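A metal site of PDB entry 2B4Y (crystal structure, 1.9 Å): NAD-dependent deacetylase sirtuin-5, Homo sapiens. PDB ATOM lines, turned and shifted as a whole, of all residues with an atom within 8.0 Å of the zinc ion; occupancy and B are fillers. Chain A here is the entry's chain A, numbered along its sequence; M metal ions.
The side-chain sulfur (SG) of Cys 176 is bound to the zinc ion, 2.1 Å away.
The side-chain sulfur (SG) of Cys 138 binds the zinc ion, at 2.3 Å.
The zinc ion is bound by SG of Cys 135 (2.4 Å).
The zinc ion is bound by the side-chain sulfur (SG) of Cys 181 (2.4 Å).
SG of Cys 176 sits close to N of Glu 178 (3.6 Å).
The backbone NH (N) of Cys 176 sits at hydrogen-bond distance from the backbone carbonyl oxygen (O) of Gly 183 (2.8 Å).
The side-chain sulfur (SG) of Cys 138 lies close to the backbone NH (N) of Val 140 (3.7 Å).
N of Ser 137 sits close to SG of Cys 135 (3.4 Å).
The backbone NH (N) of Cys 135 sits at hydrogen-bond distance from the backbone carbonyl oxygen (O) of Val 140, at 3.0 Å.
The side-chain sulfur (SG) of Cys 181 lies close to the backbone NH (N) of Gly 183 (3.4 Å).
Of the 19 residues printed, 4 come within 4 Å of the zinc ion.
The nearest printed residue that does not touch the zinc ion is Glu 178 (4.3 Å).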
ATOM      1  N   ARG A 134     -24.447  18.333   6.816  1.00  0.00           N
ATOM      2  CA  ARG A 134     -24.332  17.955   8.180  1.00  0.00           C
ATOM      3  C   ARG A 134     -25.072  18.957   9.056  1.00  0.00           C
ATOM      4  O   ARG A 134     -24.872  20.179   8.959  1.00  0.00           O
ATOM      5  CB  ARG A 134     -22.856  17.885   8.644  1.00  0.00           C
ATOM      6  CG  ARG A 134     -22.752  17.410  10.083  1.00  0.00           C
ATOM      7  CD  ARG A 134     -21.420  16.868  10.427  1.00  0.00           C
ATOM      8  NE  ARG A 134     -20.470  17.918  10.770  1.00  0.00           N
ATOM      9  CZ  ARG A 134     -19.506  18.381   9.992  1.00  0.00           C
ATOM     10  NH1 ARG A 134     -19.338  17.923   8.757  1.00  0.00           N
ATOM     11  NH2 ARG A 134     -18.686  19.325  10.467  1.00  0.00           N
ATOM     12  N   CYS A 135     -25.906  18.414   9.958  1.00  0.00           N
ATOM     13  CA  CYS A 135     -26.590  19.232  10.919  1.00  0.00           C
ATOM     14  C   CYS A 135     -25.673  19.773  12.012  1.00  0.00           C
ATOM     15  O   CYS A 135     -24.997  19.013  12.728  1.00  0.00           O
ATOM     16  CB  CYS A 135     -27.739  18.453  11.533  1.00  0.00           C
ATOM     17  SG  CYS A 135     -28.692  19.472  12.647  1.00  0.00           S
ATOM     18  N   THR A 136     -25.702  21.095  12.182  1.00  0.00           N
ATOM     19  CA  THR A 136     -24.840  21.703  13.246  1.00  0.00           C
ATOM     20  C   THR A 136     -25.319  21.422  14.674  1.00  0.00           C
ATOM     21  O   THR A 136     -24.554  21.620  15.617  1.00  0.00           O
ATOM     22  CB  THR A 136     -24.574  23.223  13.045  1.00  0.00           C
ATOM     23  OG1 THR A 136     -25.802  23.953  13.124  1.00  0.00           O
ATOM     24  CG2 THR A 136     -23.921  23.464  11.697  1.00  0.00           C
ATOM     25  N   SER A 137     -26.548  20.944  14.823  1.00  0.00           N
ATOM     26  CA  SER A 137     -27.147  20.581  16.109  1.00  0.00           C
ATOM     27  C   SER A 137     -26.965  19.114  16.475  1.00  0.00           C
ATOM     28  O   SER A 137     -26.440  18.801  17.534  1.00  0.00           O
ATOM     29  CB  SER A 137     -28.633  20.899  16.114  1.00  0.00           C
ATOM     30  OG  SER A 137     -28.804  22.188  16.647  1.00  0.00           O
ATOM     31  N   CYS A 138     -27.444  18.218  15.611  1.00  0.00           N
ATOM     32  CA  CYS A 138     -27.460  16.782  15.914  1.00  0.00           C
ATOM     33  C   CYS A 138     -26.351  15.994  15.245  1.00  0.00           C
ATOM     34  O   CYS A 138     -26.183  14.814  15.550  1.00  0.00           O
ATOM     35  CB  CYS A 138     -28.811  16.172  15.576  1.00  0.00           C
ATOM     36  SG  CYS A 138     -29.165  15.861  13.847  1.00  0.00           S
ATOM     37  N   GLY A 139     -25.627  16.591  14.304  1.00  0.00           N
ATOM     38  CA  GLY A 139     -24.500  15.915  13.661  1.00  0.00           C
ATOM     39  C   GLY A 139     -24.774  14.930  12.547  1.00  0.00           C
ATOM     40  O   GLY A 139     -23.848  14.342  11.961  1.00  0.00           O
ATOM     41  N   VAL A 140     -26.040  14.753  12.203  1.00  0.00           N
ATOM     42  CA  VAL A 140     -26.424  13.819  11.158  1.00  0.00           C
ATOM     43  C   VAL A 140     -25.959  14.292   9.760  1.00  0.00           C
ATOM     44  O   VAL A 140     -26.182  15.445   9.373  1.00  0.00           O
ATOM     45  CB  VAL A 140     -27.960  13.584  11.167  1.00  0.00           C
ATOM     46  CG1 VAL A 140     -28.458  13.129   9.800  1.00  0.00           C
ATOM     47  CG2 VAL A 140     -28.341  12.566  12.286  1.00  0.00           C
ATOM     48  N   VAL A 141     -25.347  13.403   8.997  1.00  0.00           N
ATOM     49  CA  VAL A 141     -24.941  13.707   7.640  1.00  0.00           C
ATOM     50  C   VAL A 141     -25.963  13.081   6.697  1.00  0.00           C
ATOM     51  O   VAL A 141     -26.466  11.991   6.986  1.00  0.00           O
ATOM     52  CB  VAL A 141     -23.551  13.110   7.370  1.00  0.00           C
ATOM     53  CG1 VAL A 141     -23.114  13.308   5.916  1.00  0.00           C
ATOM     54  CG2 VAL A 141     -22.523  13.747   8.321  1.00  0.00           C
ATOM     55  N   ARG A 175     -32.244  23.507   6.630  1.00  0.00           N
ATOM     56  CA  ARG A 175     -32.534  23.016   7.984  1.00  0.00           C
ATOM     57  C   ARG A 175     -32.703  21.473   8.061  1.00  0.00           C
ATOM     58  O   ARG A 175     -33.159  20.854   7.136  1.00  0.00           O
ATOM     59  CB  ARG A 175     -33.871  23.621   8.531  1.00  0.00           C
ATOM     60  CG  ARG A 175     -34.010  25.195   8.623  1.00  0.00           C
ATOM     61  CD  ARG A 175     -32.805  25.965   9.190  1.00  0.00           C
ATOM     62  NE  ARG A 175     -32.646  25.792  10.617  1.00  0.00           N
ATOM     63  CZ  ARG A 175     -32.086  26.658  11.441  1.00  0.00           C
ATOM     64  NH1 ARG A 175     -31.639  27.847  10.977  1.00  0.00           N
ATOM     65  NH2 ARG A 175     -31.974  26.356  12.728  1.00  0.00           N
ATOM     66  N   CYS A 176     -32.390  20.938   9.220  1.00  0.00           N
ATOM     67  CA  CYS A 176     -32.387  19.521   9.497  1.00  0.00           C
ATOM     68  C   CYS A 176     -33.823  18.987   9.463  1.00  0.00           C
ATOM     69  O   CYS A 176     -34.698  19.561  10.125  1.00  0.00           O
ATOM     70  CB  CYS A 176     -31.773  19.320  10.886  1.00  0.00           C
ATOM     71  SG  CYS A 176     -31.404  17.546  11.392  1.00  0.00           S
ATOM     72  N   GLU A 177     -34.066  17.904   8.721  1.00  0.00           N
ATOM     73  CA  GLU A 177     -35.359  17.237   8.759  1.00  0.00           C
ATOM     74  C   GLU A 177     -35.487  16.101   9.789  1.00  0.00           C
ATOM     75  O   GLU A 177     -36.522  15.440   9.798  1.00  0.00           O
ATOM     76  CB  GLU A 177     -35.771  16.773   7.358  1.00  0.00           C
ATOM     77  CG  GLU A 177     -35.934  17.913   6.378  1.00  0.00           C
ATOM     78  CD  GLU A 177     -35.933  17.448   4.930  1.00  0.00           C
ATOM     79  OE1 GLU A 177     -35.366  16.344   4.624  1.00  0.00           O
ATOM     80  OE2 GLU A 177     -36.484  18.205   4.094  1.00  0.00           O
ATOM     81  N   GLU A 178     -34.493  15.890  10.648  1.00  0.00           N
ATOM     82  CA  GLU A 178     -34.616  14.875  11.702  1.00  0.00           C
ATOM     83  C   GLU A 178     -35.755  15.288  12.637  1.00  0.00           C
ATOM     84  O   GLU A 178     -35.944  16.491  12.912  1.00  0.00           O
ATOM     85  CB  GLU A 178     -33.319  14.720  12.510  1.00  0.00           C
ATOM     86  CG  GLU A 178     -32.091  14.201  11.764  1.00  0.00           C
ATOM     87  CD  GLU A 178     -32.116  12.721  11.497  1.00  0.00           C
ATOM     88  OE1 GLU A 178     -32.068  11.948  12.479  1.00  0.00           O
ATOM     89  OE2 GLU A 178     -32.163  12.320  10.318  1.00  0.00           O
ATOM     90  N   ALA A 179     -36.538  14.311  13.118  1.00  0.00           N
ATOM     91  CA  ALA A 179     -37.750  14.641  13.891  1.00  0.00           C
ATOM     92  C   ALA A 179     -37.417  15.416  15.152  1.00  0.00           C
ATOM     93  O   ALA A 179     -36.606  14.996  15.956  1.00  0.00           O
ATOM     94  CB  ALA A 179     -38.556  13.364  14.217  1.00  0.00           C
ATOM     95  N   GLY A 180     -37.992  16.601  15.300  1.00  0.00           N
ATOM     96  CA  GLY A 180     -37.700  17.382  16.515  1.00  0.00           C
ATOM     97  C   GLY A 180     -36.356  18.115  16.571  1.00  0.00           C
ATOM     98  O   GLY A 180     -36.044  18.746  17.603  1.00  0.00           O
ATOM     99  N   CYS A 181     -35.550  18.076  15.491  1.00  0.00           N
ATOM    100  CA  CYS A 181     -34.263  18.766  15.516  1.00  0.00           C
ATOM    101  C   CYS A 181     -34.329  20.234  15.108  1.00  0.00           C
ATOM    102  O   CYS A 181     -33.986  21.111  15.896  1.00  0.00           O
ATOM    103  CB  CYS A 181     -33.188  18.066  14.670  1.00  0.00           C
ATOM    104  SG  CYS A 181     -31.613  18.974  14.835  1.00  0.00           S
ATOM    105  N   GLY A 182     -34.681  20.470  13.842  1.00  0.00           N
ATOM    106  CA  GLY A 182     -34.837  21.807  13.300  1.00  0.00           C
ATOM    107  C   GLY A 182     -33.532  22.607  13.135  1.00  0.00           C
ATOM    108  O   GLY A 182     -33.589  23.779  12.817  1.00  0.00           O
ATOM    109  N   GLY A 183     -32.370  21.971  13.335  1.00  0.00           N
ATOM    110  CA  GLY A 183     -31.080  22.670  13.346  1.00  0.00           C
ATOM    111  C   GLY A 183     -30.639  23.225  11.982  1.00  0.00           C
ATOM    112  O   GLY A 183     -31.087  22.780  10.942  1.00  0.00           O
ATOM    113  N   LEU A 184     -29.721  24.196  12.027  1.00  0.00           N
ATOM    114  CA  LEU A 184     -29.009  24.688  10.836  1.00  0.00           C
ATOM    115  C   LEU A 184     -28.034  23.642  10.277  1.00  0.00           C
ATOM    116  O   LEU A 184     -27.115  23.188  10.975  1.00  0.00           O
ATOM    117  CB  LEU A 184     -28.196  25.956  11.206  1.00  0.00           C
ATOM    118  CG  LEU A 184     -27.520  26.658  10.011  1.00  0.00           C
ATOM    119  CD1 LEU A 184     -28.465  26.898   8.756  1.00  0.00           C
ATOM    120  CD2 LEU A 184     -26.776  27.935  10.403  1.00  0.00           C
ATOM    121  N   LEU A 185     -28.195  23.342   8.997  1.00  0.00           N
ATOM    122  CA  LEU A 185     -27.261  22.523   8.230  1.00  0.00           C
ATOM    123  C   LEU A 185     -26.076  23.339   7.723  1.00  0.00           C
ATOM    124  O   LEU A 185     -26.175  24.538   7.539  1.00  0.00           O
ATOM    125  CB  LEU A 185     -27.948  21.883   7.051  1.00  0.00           C
ATOM    126  CG  LEU A 185     -29.216  21.072   7.361  1.00  0.00           C
ATOM    127  CD1 LEU A 185     -29.718  20.546   5.989  1.00  0.00           C
ATOM    128  CD2 LEU A 185     -28.912  19.922   8.284  1.00  0.00           C
HETATM  129 ZN    ZN M   1     -30.277  17.815  13.198  1.00  0.00          ZN
